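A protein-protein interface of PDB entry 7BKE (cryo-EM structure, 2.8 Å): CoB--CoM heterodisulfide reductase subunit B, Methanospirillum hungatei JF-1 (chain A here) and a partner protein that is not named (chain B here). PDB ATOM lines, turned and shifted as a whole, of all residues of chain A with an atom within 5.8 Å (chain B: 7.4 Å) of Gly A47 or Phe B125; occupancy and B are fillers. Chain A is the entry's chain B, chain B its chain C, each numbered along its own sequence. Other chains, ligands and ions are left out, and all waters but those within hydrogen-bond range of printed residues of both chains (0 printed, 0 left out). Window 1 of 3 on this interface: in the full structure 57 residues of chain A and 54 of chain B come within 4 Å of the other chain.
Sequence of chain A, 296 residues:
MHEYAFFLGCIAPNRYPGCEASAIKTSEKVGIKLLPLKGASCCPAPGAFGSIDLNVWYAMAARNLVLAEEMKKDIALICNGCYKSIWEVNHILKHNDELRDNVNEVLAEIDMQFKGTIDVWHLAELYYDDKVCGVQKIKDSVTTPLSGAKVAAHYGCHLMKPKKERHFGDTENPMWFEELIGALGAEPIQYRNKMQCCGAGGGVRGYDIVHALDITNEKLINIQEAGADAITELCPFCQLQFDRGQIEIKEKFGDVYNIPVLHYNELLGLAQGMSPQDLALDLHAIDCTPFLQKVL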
ATOM      1  N   PRO A  44     -12.618   3.533  10.800  1.00  0.00           N
ATOM      2  CA  PRO A  44     -13.471   2.383  11.077  1.00  0.00           C
ATOM      3  C   PRO A  44     -12.970   1.257  10.194  1.00  0.00           C
ATOM      4  O   PRO A  44     -13.114   1.307   8.971  1.00  0.00           O
ATOM      5  CB  PRO A  44     -14.866   2.879  10.703  1.00  0.00           C
ATOM      6  CG  PRO A  44     -14.622   3.985   9.759  1.00  0.00           C
ATOM      7  CD  PRO A  44     -13.324   4.609  10.100  1.00  0.00           C
ATOM      8  N   ALA A  45     -12.343   0.263  10.818  1.00  0.00           N
ATOM      9  CA  ALA A  45     -11.573  -0.719  10.074  1.00  0.00           C
ATOM     10  C   ALA A  45     -12.476  -1.395   9.055  1.00  0.00           C
ATOM     11  O   ALA A  45     -13.553  -1.877   9.419  1.00  0.00           O
ATOM     12  CB  ALA A  45     -10.957  -1.752  11.008  1.00  0.00           C
ATOM     13  N   PRO A  46     -12.092  -1.427   7.783  1.00  0.00           N
ATOM     14  CA  PRO A  46     -13.079  -1.733   6.737  1.00  0.00           C
ATOM     15  C   PRO A  46     -13.726  -3.096   6.885  1.00  0.00           C
ATOM     16  O   PRO A  46     -14.917  -3.244   6.594  1.00  0.00           O
ATOM     17  CB  PRO A  46     -12.260  -1.620   5.449  1.00  0.00           C
ATOM     18  CG  PRO A  46     -10.854  -1.784   5.862  1.00  0.00           C
ATOM     19  CD  PRO A  46     -10.726  -1.309   7.260  1.00  0.00           C
ATOM     20  N   GLY A  47     -12.985  -4.095   7.344  1.00  0.00           N
ATOM     21  CA  GLY A  47     -13.563  -5.410   7.497  1.00  0.00           C
ATOM     22  C   GLY A  47     -14.402  -5.536   8.748  1.00  0.00           C
ATOM     23  O   GLY A  47     -15.621  -5.716   8.676  1.00  0.00           O
ATOM     24  N   ALA A  48     -13.758  -5.391   9.901  1.00  0.00           N
ATOM     25  CA  ALA A  48     -14.401  -5.676  11.173  1.00  0.00           C
ATOM     26  C   ALA A  48     -15.487  -4.678  11.537  1.00  0.00           C
ATOM     27  O   ALA A  48     -16.172  -4.883  12.544  1.00  0.00           O
ATOM     28  CB  ALA A  48     -13.356  -5.714  12.283  1.00  0.00           C
ATOM     29  N   PHE A  49     -15.653  -3.606  10.771  1.00  0.00           N
ATOM     30  CA  PHE A  49     -16.604  -2.582  11.164  1.00  0.00           C
ATOM     31  C   PHE A  49     -17.537  -2.275   9.998  1.00  0.00           C
ATOM     32  O   PHE A  49     -18.734  -2.000  10.180  1.00  0.00           O
ATOM     33  CB  PHE A  49     -15.833  -1.354  11.639  1.00  0.00           C
ATOM     34  CG  PHE A  49     -16.598  -0.483  12.564  1.00  0.00           C
ATOM     35  CD1 PHE A  49     -16.462  -0.646  13.926  1.00  0.00           C
ATOM     36  CD2 PHE A  49     -17.424   0.508  12.094  1.00  0.00           C
ATOM     37  CE1 PHE A  49     -17.154   0.142  14.800  1.00  0.00           C
ATOM     38  CE2 PHE A  49     -18.105   1.304  12.972  1.00  0.00           C
ATOM     39  CZ  PHE A  49     -17.974   1.119  14.324  1.00  0.00           C
ATOM     40  N   GLY A  50     -16.986  -2.336   8.786  1.00  0.00           N
ATOM     41  CA  GLY A  50     -17.818  -2.291   7.601  1.00  0.00           C
ATOM     42  C   GLY A  50     -18.717  -3.498   7.470  1.00  0.00           C
ATOM     43  O   GLY A  50     -19.829  -3.390   6.948  1.00  0.00           O
ATOM     44  N   SER A  51     -18.256  -4.666   7.927  1.00  0.00           N
ATOM     45  CA  SER A  51     -19.108  -5.846   7.923  1.00  0.00           C
ATOM     46  C   SER A  51     -20.311  -5.664   8.836  1.00  0.00           C
ATOM     47  O   SER A  51     -21.371  -6.242   8.584  1.00  0.00           O
ATOM     48  CB  SER A  51     -18.310  -7.070   8.351  1.00  0.00           C
ATOM     49  OG  SER A  51     -17.179  -7.246   7.521  1.00  0.00           O
ATOM     50  N   ILE A  52     -20.171  -4.874   9.888  1.00  0.00           N
ATOM     51  CA  ILE A  52     -21.268  -4.662  10.818  1.00  0.00           C
ATOM     52  C   ILE A  52     -22.221  -3.596  10.312  1.00  0.00           C
ATOM     53  O   ILE A  52     -23.429  -3.828  10.217  1.00  0.00           O
ATOM     54  CB  ILE A  52     -20.721  -4.294  12.206  1.00  0.00           C
ATOM     55  CG1 ILE A  52     -19.897  -5.433  12.779  1.00  0.00           C
ATOM     56  CG2 ILE A  52     -21.848  -4.000  13.135  1.00  0.00           C
ATOM     57  CD1 ILE A  52     -19.140  -5.015  14.003  1.00  0.00           C
ATOM     58  N   HIS A 158      -5.902  -3.967  -0.251  1.00  0.00           N
ATOM     59  CA  HIS A 158      -6.751  -2.792  -0.185  1.00  0.00           C
ATOM     60  C   HIS A 158      -6.102  -1.554  -0.772  1.00  0.00           C
ATOM     61  O   HIS A 158      -6.803  -0.570  -1.015  1.00  0.00           O
ATOM     62  CB  HIS A 158      -7.158  -2.542   1.257  1.00  0.00           C
ATOM     63  CG  HIS A 158      -8.086  -3.578   1.793  1.00  0.00           C
ATOM     64  ND1 HIS A 158      -8.162  -3.891   3.131  1.00  0.00           N
ATOM     65  CD2 HIS A 158      -8.979  -4.379   1.169  1.00  0.00           C
ATOM     66  CE1 HIS A 158      -9.063  -4.839   3.306  1.00  0.00           C
ATOM     67  NE2 HIS A 158      -9.573  -5.150   2.131  1.00  0.00           N
ATOM     68  N   GLY A 201      -7.797  -9.983   6.255  1.00  0.00           N
ATOM     69  CA  GLY A 201      -8.790  -8.980   5.955  1.00  0.00           C
ATOM     70  C   GLY A 201     -10.189  -9.434   6.294  1.00  0.00           C
ATOM     71  O   GLY A 201     -10.454 -10.599   6.573  1.00  0.00           O
ATOM     72  N   GLY A 202     -11.107  -8.475   6.288  1.00  0.00           N
ATOM     73  CA  GLY A 202     -12.516  -8.765   6.429  1.00  0.00           C
ATOM     74  C   GLY A 202     -12.954  -9.302   7.768  1.00  0.00           C
ATOM     75  O   GLY A 202     -14.096  -9.746   7.894  1.00  0.00           O
ATOM     76  N   GLY A 203     -12.095  -9.271   8.780  1.00  0.00           N
ATOM     77  CA  GLY A 203     -12.426  -9.864  10.052  1.00  0.00           C
ATOM     78  C   GLY A 203     -12.207 -11.354  10.141  1.00  0.00           C
ATOM     79  O   GLY A 203     -12.544 -11.950  11.168  1.00  0.00           O
ATOM     80  N   VAL A 204     -11.661 -11.978   9.100  1.00  0.00           N
ATOM     81  CA  VAL A 204     -11.410 -13.413   9.139  1.00  0.00           C
ATOM     82  C   VAL A 204     -10.360 -13.734  10.192  1.00  0.00           C
ATOM     83  O   VAL A 204     -10.448 -14.755  10.884  1.00  0.00           O
ATOM     84  CB  VAL A 204     -10.999 -13.914   7.743  1.00  0.00           C
ATOM     85  CG1 VAL A 204     -10.625 -15.370   7.788  1.00  0.00           C
ATOM     86  CG2 VAL A 204     -12.118 -13.683   6.765  1.00  0.00           C
ATOM     87  N   TYR A 207     -12.566 -14.108  13.152  1.00  0.00           N
ATOM     88  CA  TYR A 207     -13.649 -15.082  13.089  1.00  0.00           C
ATOM     89  C   TYR A 207     -13.123 -16.510  13.009  1.00  0.00           C
ATOM     90  O   TYR A 207     -13.570 -17.382  13.760  1.00  0.00           O
ATOM     91  CB  TYR A 207     -14.552 -14.780  11.898  1.00  0.00           C
ATOM     92  CG  TYR A 207     -15.502 -15.901  11.576  1.00  0.00           C
ATOM     93  CD1 TYR A 207     -16.534 -16.227  12.437  1.00  0.00           C
ATOM     94  CD2 TYR A 207     -15.362 -16.641  10.417  1.00  0.00           C
ATOM     95  CE1 TYR A 207     -17.405 -17.249  12.147  1.00  0.00           C
ATOM     96  CE2 TYR A 207     -16.226 -17.664  10.120  1.00  0.00           C
ATOM     97  CZ  TYR A 207     -17.246 -17.964  10.988  1.00  0.00           C
ATOM     98  OH  TYR A 207     -18.112 -18.990  10.692  1.00  0.00           O
ATOM     99  N   TRP B  86     -18.814 -15.295   6.643  1.00  0.00           N
ATOM    100  CA  TRP B  86     -17.776 -14.566   7.343  1.00  0.00           C
ATOM    101  C   TRP B  86     -16.387 -15.074   6.999  1.00  0.00           C
ATOM    102  O   TRP B  86     -15.431 -14.788   7.720  1.00  0.00           O
ATOM    103  CB  TRP B  86     -18.030 -14.642   8.844  1.00  0.00           C
ATOM    104  CG  TRP B  86     -19.463 -14.424   9.173  1.00  0.00           C
ATOM    105  CD1 TRP B  86     -20.422 -15.370   9.299  1.00  0.00           C
ATOM    106  CD2 TRP B  86     -20.108 -13.170   9.396  1.00  0.00           C
ATOM    107  NE1 TRP B  86     -21.627 -14.789   9.589  1.00  0.00           N
ATOM    108  CE2 TRP B  86     -21.458 -13.435   9.653  1.00  0.00           C
ATOM    109  CE3 TRP B  86     -19.672 -11.846   9.405  1.00  0.00           C
ATOM    110  CZ2 TRP B  86     -22.371 -12.433   9.917  1.00  0.00           C
ATOM    111  CZ3 TRP B  86     -20.576 -10.859   9.663  1.00  0.00           C
ATOM    112  CH2 TRP B  86     -21.911 -11.153   9.922  1.00  0.00           C
ATOM    113  N   CYS B  88     -15.122 -14.374   3.900  1.00  0.00           N
ATOM    114  CA  CYS B  88     -14.620 -13.454   2.892  1.00  0.00           C
ATOM    115  C   CYS B  88     -13.613 -12.508   3.534  1.00  0.00           C
ATOM    116  O   CYS B  88     -13.926 -11.838   4.519  1.00  0.00           O
ATOM    117  CB  CYS B  88     -15.773 -12.675   2.266  1.00  0.00           C
ATOM    118  SG  CYS B  88     -15.298 -11.446   1.052  1.00  0.00           S
ATOM    119  N   THR B  89     -12.407 -12.452   2.983  1.00  0.00           N
ATOM    120  CA  THR B  89     -11.393 -11.528   3.458  1.00  0.00           C
ATOM    121  C   THR B  89     -11.504 -10.156   2.819  1.00  0.00           C
ATOM    122  O   THR B  89     -10.689  -9.282   3.125  1.00  0.00           O
ATOM    123  CB  THR B  89      -9.994 -12.081   3.205  1.00  0.00           C
ATOM    124  OG1 THR B  89      -9.774 -12.200   1.799  1.00  0.00           O
ATOM    125  CG2 THR B  89      -9.832 -13.433   3.847  1.00  0.00           C
ATOM    126  N   THR B  90     -12.485  -9.949   1.947  1.00  0.00           N
ATOM    127  CA  THR B  90     -12.640  -8.707   1.196  1.00  0.00           C
ATOM    128  C   THR B  90     -11.351  -8.334   0.470  1.00  0.00           C
ATOM    129  O   THR B  90     -10.929  -7.181   0.454  1.00  0.00           O
ATOM    130  CB  THR B  90     -13.122  -7.575   2.096  1.00  0.00           C
ATOM    131  OG1 THR B  90     -12.072  -7.182   2.978  1.00  0.00           O
ATOM    132  CG2 THR B  90     -14.311  -8.025   2.910  1.00  0.00           C
ATOM    133  N   MET B 109     -20.737  -7.707   1.766  1.00  0.00           N
ATOM    134  CA  MET B 109     -20.794  -6.722   2.841  1.00  0.00           C
ATOM    135  C   MET B 109     -22.236  -6.365   3.182  1.00  0.00           C
ATOM    136  O   MET B 109     -22.607  -6.280   4.360  1.00  0.00           O
ATOM    137  CB  MET B 109     -20.015  -5.477   2.431  1.00  0.00           C
ATOM    138  CG  MET B 109     -18.533  -5.727   2.255  1.00  0.00           C
ATOM    139  SD  MET B 109     -17.639  -6.297   3.696  1.00  0.00           S
ATOM    140  CE  MET B 109     -17.689  -4.824   4.689  1.00  0.00           C
ATOM    141  N   ARG B 112     -23.743  -9.172   5.112  1.00  0.00           N
ATOM    142  CA  ARG B 112     -23.287  -9.163   6.496  1.00  0.00           C
ATOM    143  C   ARG B 112     -24.034  -8.121   7.313  1.00  0.00           C
ATOM    144  O   ARG B 112     -24.348  -8.350   8.485  1.00  0.00           O
ATOM    145  CB  ARG B 112     -21.786  -8.913   6.555  1.00  0.00           C
ATOM    146  CG  ARG B 112     -20.944 -10.119   6.225  1.00  0.00           C
ATOM    147  CD  ARG B 112     -19.487  -9.759   6.176  1.00  0.00           C
ATOM    148  NE  ARG B 112     -18.658 -10.873   5.755  1.00  0.00           N
ATOM    149  CZ  ARG B 112     -17.342 -10.911   5.897  1.00  0.00           C
ATOM    150  NH1 ARG B 112     -16.707  -9.901   6.450  1.00  0.00           N
ATOM    151  NH2 ARG B 112     -16.659 -11.961   5.486  1.00  0.00           N
ATOM    152  N   PHE B 116     -26.281  -8.956  10.583  1.00  0.00           N
ATOM    153  CA  PHE B 116     -26.177  -8.279  11.870  1.00  0.00           C
ATOM    154  C   PHE B 116     -27.529  -7.745  12.317  1.00  0.00           C
ATOM    155  O   PHE B 116     -27.887  -7.860  13.493  1.00  0.00           O
ATOM    156  CB  PHE B 116     -25.157  -7.146  11.812  1.00  0.00           C
ATOM    157  CG  PHE B 116     -25.049  -6.370  13.097  1.00  0.00           C
ATOM    158  CD1 PHE B 116     -24.194  -6.783  14.098  1.00  0.00           C
ATOM    159  CD2 PHE B 116     -25.803  -5.231  13.304  1.00  0.00           C
ATOM    160  CE1 PHE B 116     -24.093  -6.080  15.280  1.00  0.00           C
ATOM    161  CE2 PHE B 116     -25.707  -4.526  14.486  1.00  0.00           C
ATOM    162  CZ  PHE B 116     -24.852  -4.951  15.473  1.00  0.00           C
ATOM    163  N   VAL B 121     -24.018 -12.738  13.984  1.00  0.00           N
ATOM    164  CA  VAL B 121     -22.752 -12.013  13.894  1.00  0.00           C
ATOM    165  C   VAL B 121     -21.726 -12.651  14.824  1.00  0.00           C
ATOM    166  O   VAL B 121     -22.049 -12.991  15.968  1.00  0.00           O
ATOM    167  CB  VAL B 121     -22.958 -10.516  14.190  1.00  0.00           C
ATOM    168  CG1 VAL B 121     -23.436 -10.300  15.608  1.00  0.00           C
ATOM    169  CG2 VAL B 121     -21.691  -9.736  13.922  1.00  0.00           C
ATOM    170  N   PRO B 122     -20.499 -12.869  14.365  1.00  0.00           N
ATOM    171  CA  PRO B 122     -19.460 -13.395  15.254  1.00  0.00           C
ATOM    172  C   PRO B 122     -19.085 -12.398  16.336  1.00  0.00           C
ATOM    173  O   PRO B 122     -19.258 -11.188  16.201  1.00  0.00           O
ATOM    174  CB  PRO B 122     -18.283 -13.652  14.307  1.00  0.00           C
ATOM    175  CG  PRO B 122     -18.905 -13.802  12.978  1.00  0.00           C
ATOM    176  CD  PRO B 122     -20.076 -12.883  12.959  1.00  0.00           C
ATOM    177  N   LYS B 123     -18.544 -12.935  17.431  1.00  0.00           N
ATOM    178  CA  LYS B 123     -18.322 -12.145  18.633  1.00  0.00           C
ATOM    179  C   LYS B 123     -17.131 -11.201  18.538  1.00  0.00           C
ATOM    180  O   LYS B 123     -17.087 -10.218  19.283  1.00  0.00           O
ATOM    181  CB  LYS B 123     -18.149 -13.069  19.834  1.00  0.00           C
ATOM    182  CG  LYS B 123     -19.338 -13.968  20.058  1.00  0.00           C
ATOM    183  CD  LYS B 123     -20.567 -13.157  20.420  1.00  0.00           C
ATOM    184  CE  LYS B 123     -21.822 -14.007  20.366  1.00  0.00           C
ATOM    185  NZ  LYS B 123     -22.887 -13.512  21.282  1.00  0.00           N
ATOM    186  N   ASN B 124     -16.166 -11.471  17.661  1.00  0.00           N
ATOM    187  CA  ASN B 124     -15.048 -10.543  17.514  1.00  0.00           C
ATOM    188  C   ASN B 124     -15.530  -9.186  17.027  1.00  0.00           C
ATOM    189  O   ASN B 124     -15.003  -8.144  17.430  1.00  0.00           O
ATOM    190  CB  ASN B 124     -14.008 -11.109  16.552  1.00  0.00           C
ATOM    191  CG  ASN B 124     -14.600 -11.500  15.216  1.00  0.00           C
ATOM    192  OD1 ASN B 124     -15.793 -11.736  15.105  1.00  0.00           O
ATOM    193  ND2 ASN B 124     -13.770 -11.533  14.188  1.00  0.00           N
ATOM    194  N   PHE B 125     -16.532  -9.182  16.151  1.00  0.00           N
ATOM    195  CA  PHE B 125     -17.088  -7.931  15.660  1.00  0.00           C
ATOM    196  C   PHE B 125     -17.684  -7.117  16.801  1.00  0.00           C
ATOM    197  O   PHE B 125     -17.437  -5.908  16.917  1.00  0.00           O
ATOM    198  CB  PHE B 125     -18.136  -8.235  14.591  1.00  0.00           C
ATOM    199  CG  PHE B 125     -17.571  -8.840  13.345  1.00  0.00           C
ATOM    200  CD1 PHE B 125     -16.985  -8.052  12.379  1.00  0.00           C
ATOM    201  CD2 PHE B 125     -17.623 -10.200  13.138  1.00  0.00           C
ATOM    202  CE1 PHE B 125     -16.468  -8.611  11.235  1.00  0.00           C
ATOM    203  CE2 PHE B 125     -17.103 -10.759  11.998  1.00  0.00           C
ATOM    204  CZ  PHE B 125     -16.526  -9.964  11.048  1.00  0.00           C
ATOM    205  N   LEU B 126     -18.452  -7.768  17.671  1.00  0.00           N
ATOM    206  CA  LEU B 126     -19.048  -7.072  18.806  1.00  0.00           C
ATOM    207  C   LEU B 126     -17.984  -6.583  19.778  1.00  0.00           C
ATOM    208  O   LEU B 126     -18.101  -5.486  20.336  1.00  0.00           O
ATOM    209  CB  LEU B 126     -20.043  -7.987  19.508  1.00  0.00           C
ATOM    210  CG  LEU B 126     -21.014  -8.705  18.579  1.00  0.00           C
ATOM    211  CD1 LEU B 126     -21.856  -9.687  19.354  1.00  0.00           C
ATOM    212  CD2 LEU B 126     -21.890  -7.701  17.855  1.00  0.00           C
ATOM    213  N   GLN B 127     -16.938  -7.377  19.998  1.00  0.00           N
ATOM    214  CA  GLN B 127     -15.869  -6.942  20.890  1.00  0.00           C
ATOM    215  C   GLN B 127     -15.140  -5.729  20.327  1.00  0.00           C
ATOM    216  O   GLN B 127     -14.765  -4.816  21.073  1.00  0.00           O
ATOM    217  CB  GLN B 127     -14.902  -8.091  21.147  1.00  0.00           C
ATOM    218  CG  GLN B 127     -15.449  -9.133  22.103  1.00  0.00           C
ATOM    219  CD  GLN B 127     -14.692 -10.442  22.031  1.00  0.00           C
ATOM    220  OE1 GLN B 127     -14.068 -10.758  21.020  1.00  0.00           O
ATOM    221  NE2 GLN B 127     -14.752 -11.217  23.105  1.00  0.00           N
ATOM    222  N   THR B 128     -14.928  -5.701  19.012  1.00  0.00           N
ATOM    223  CA  THR B 128     -14.336  -4.526  18.384  1.00  0.00           C
ATOM    224  C   THR B 128     -15.236  -3.311  18.538  1.00  0.00           C
ATOM    225  O   THR B 128     -14.753  -2.191  18.755  1.00  0.00           O
ATOM    226  CB  THR B 128     -14.059  -4.809  16.909  1.00  0.00           C
ATOM    227  OG1 THR B 128     -12.935  -5.688  16.800  1.00  0.00           O
ATOM    228  CG2 THR B 128     -13.765  -3.530  16.157  1.00  0.00           C
ATOM    229  N   VAL B 129     -16.550  -3.507  18.427  1.00  0.00           N
ATOM    230  CA  VAL B 129     -17.477  -2.407  18.673  1.00  0.00           C
ATOM    231  C   VAL B 129     -17.305  -1.877  20.090  1.00  0.00           C
ATOM    232  O   VAL B 129     -17.267  -0.662  20.311  1.00  0.00           O
ATOM    233  CB  VAL B 129     -18.925  -2.853  18.411  1.00  0.00           C
ATOM    234  CG1 VAL B 129     -19.894  -1.932  19.113  1.00  0.00           C
ATOM    235  CG2 VAL B 129     -19.203  -2.864  16.931  1.00  0.00           C
ATOM    236  N   GLN B 130     -17.194  -2.777  21.067  1.00  0.00           N
ATOM    237  CA  GLN B 130     -17.005  -2.343  22.451  1.00  0.00           C
ATOM    238  C   GLN B 130     -15.721  -1.541  22.604  1.00  0.00           C
ATOM    239  O   GLN B 130     -15.707  -0.491  23.260  1.00  0.00           O
ATOM    240  CB  GLN B 130     -16.973  -3.546  23.395  1.00  0.00           C
ATOM    241  CG  GLN B 130     -18.110  -4.528  23.230  1.00  0.00           C
ATOM    242  CD  GLN B 130     -19.374  -4.081  23.915  1.00  0.00           C
ATOM    243  OE1 GLN B 130     -19.361  -3.687  25.076  1.00  0.00           O
ATOM    244  NE2 GLN B 130     -20.485  -4.143  23.192  1.00  0.00           N
ATOM    245  N   LEU B 131     -14.629  -2.026  22.012  1.00  0.00           N
ATOM    246  CA  LEU B 131     -13.345  -1.340  22.135  1.00  0.00           C
ATOM    247  C   LEU B 131     -13.391   0.047  21.508  1.00  0.00           C
ATOM    248  O   LEU B 131     -12.875   1.013  22.080  1.00  0.00           O
ATOM    249  CB  LEU B 131     -12.241  -2.167  21.485  1.00  0.00           C
ATOM    250  CG  LEU B 131     -11.821  -3.449  22.194  1.00  0.00           C
ATOM    251  CD1 LEU B 131     -11.210  -4.411  21.201  1.00  0.00           C
ATOM    252  CD2 LEU B 131     -10.844  -3.132  23.305  1.00  0.00           C
ATOM    253  N   ILE B 132     -13.985   0.159  20.321  1.00  0.00           N
ATOM    254  CA  ILE B 132     -14.042   1.450  19.646  1.00  0.00           C
ATOM    255  C   ILE B 132     -14.954   2.405  20.404  1.00  0.00           C
ATOM    256  O   ILE B 132     -14.688   3.610  20.478  1.00  0.00           O
ATOM    257  CB  ILE B 132     -14.481   1.265  18.184  1.00  0.00           C
ATOM    258  CG1 ILE B 132     -13.309   0.764  17.348  1.00  0.00           C
ATOM    259  CG2 ILE B 132     -14.992   2.560  17.603  1.00  0.00           C
ATOM    260  CD1 ILE B 132     -13.706   0.224  16.007  1.00  0.00           C
ATOM    261  N   LEU B 180     -25.458   0.967  17.506  1.00  0.00           N
ATOM    262  CA  LEU B 180     -24.547  -0.150  17.354  1.00  0.00           C
ATOM    263  C   LEU B 180     -24.160  -0.732  18.704  1.00  0.00           C
ATOM    264  O   LEU B 180     -24.122  -1.954  18.869  1.00  0.00           O
ATOM    265  CB  LEU B 180     -23.315   0.308  16.583  1.00  0.00           C
ATOM    266  CG  LEU B 180     -22.413  -0.809  16.101  1.00  0.00           C
ATOM    267  CD1 LEU B 180     -23.280  -1.789  15.379  1.00  0.00           C
ATOM    268  CD2 LEU B 180     -21.355  -0.258  15.182  1.00  0.00           C
ATOM    269  N   ALA B 184     -24.889  -4.418  20.130  1.00  0.00           N
ATOM    270  CA  ALA B 184     -23.749  -5.286  20.388  1.00  0.00           C
ATOM    271  C   ALA B 184     -23.772  -5.826  21.810  1.00  0.00           C
ATOM    272  O   ALA B 184     -23.536  -7.019  22.027  1.00  0.00           O
ATOM    273  CB  ALA B 184     -22.446  -4.537  20.122  1.00  0.00           C
ATOM    274  N   LEU B 188     -24.206  -9.733  22.848  1.00  0.00           N
ATOM    275  CA  LEU B 188     -23.185 -10.350  23.686  1.00  0.00           C
ATOM    276  C   LEU B 188     -23.778 -10.946  24.956  1.00  0.00           C
ATOM    277  O   LEU B 188     -23.286 -11.969  25.446  1.00  0.00           O
ATOM    278  CB  LEU B 188     -22.110  -9.324  24.038  1.00  0.00           C
ATOM    279  CG  LEU B 188     -20.920  -9.227  23.086  1.00  0.00           C
ATOM    280  CD1 LEU B 188     -20.172  -7.925  23.301  1.00  0.00           C
ATOM    281  CD2 LEU B 188     -19.995 -10.408  23.281  1.00  0.00           C
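ND2 of Asn B124 lies within hydrogen-bond range of O of Gly A203, at 3.3 Å.
The backbone NH of Tyr A207 sits close to the side-chain amide nitrogen of Asn B124 (3.0 Å).
O of Thr B89 is in hydrogen-bond range of N of Gly A202 (3.3 Å).
The side-chain hydroxyl of Ser A51 is in hydrogen-bond range of the guanidinium group of Arg B112 (2.9 Å).
A ring nitrogen (NE2) of His A158 is in hydrogen-bond range of the backbone carbonyl oxygen of Thr B90 (3.0 Å).
The backbone carbonyl oxygen of Gly A202 is in hydrogen-bond range of the guanidinium group of Arg B112, 3.0 Å away.
O of Asn B124 lies within hydrogen-bond range of OG1 of Thr B128, at 3.3 Å.
OG of Ser A51 sits at hydrogen-bond distance from O of Gly A47.
O of Cys B88 lies within hydrogen-bond range of NH2 of Arg B112.
The side-chain sulfur (SG) of Cys B88 lies close to the backbone NH (N) of Thr B90, at 3.3 Å.
Met B109 touches Pro A46 (CE to O, 3.7 Å).
Leu B180 touches Phe A49 (CD2 to CZ, 3.8 Å).
Ser A51 touches Met B109.
Phe B125 touches Ile A52.
Ile A52 touches Leu B180.
Thr B90 touches Gly A202 (OG1 to N, 3.7 Å).
Gly A202 touches Phe B125 (O to CZ, 3.99 Å).
CG2 of Val A204 touches O of Trp B86, 3.6 Å away.
CG2 of Val A204 touches O of Cys B88, 3.4 Å away.
CG of Pro B122 touches CD1 of Tyr A207, 3.4 Å away.
Gly A47 touches just one residue of chain B: Phe B125.
Printed residues of chain A within 4 Å of Phe B125: Gly A47, Ala A48, Ser A51, Ile A52 and Gly A202.
Printed residues of chain B within 4 Å of Ile A52: Phe B116 (3.7 Å), Phe B125 (3.4 Å), Val B129 (3.6 Å) and Leu B180 (3.5 Å).
Printed residues of chain B within 4 Å of Ser A51: Met B109 (3.3 Å), Arg B112 (2.9 Å) and Phe B125 (3.8 Å).
Leu B131 touches none of the printed residues of chain A.
Printed residues of chain A that touch a printed residue of chain B: Pro A46, Gly A47, Ala A48, Phe A49, Gly A50, Ser A51, Ile A52, His A158, Gly A201, Gly A202, Gly A203, Val A204 and Tyr A207.
Hydrophobic or aromatic side chains of chain A that line the printed part of chain B: Phe A49, Ile A52, His A158, Val A204 and Tyr A207.
Printed residues of chain B that touch a printed residue of chain A: Trp B86, Cys B88, Thr B89, Thr B90, Met B109, Arg B112, Phe B116, Pro B122, Asn B124, Phe B125, Val B129, Ile B132 and Leu B180.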
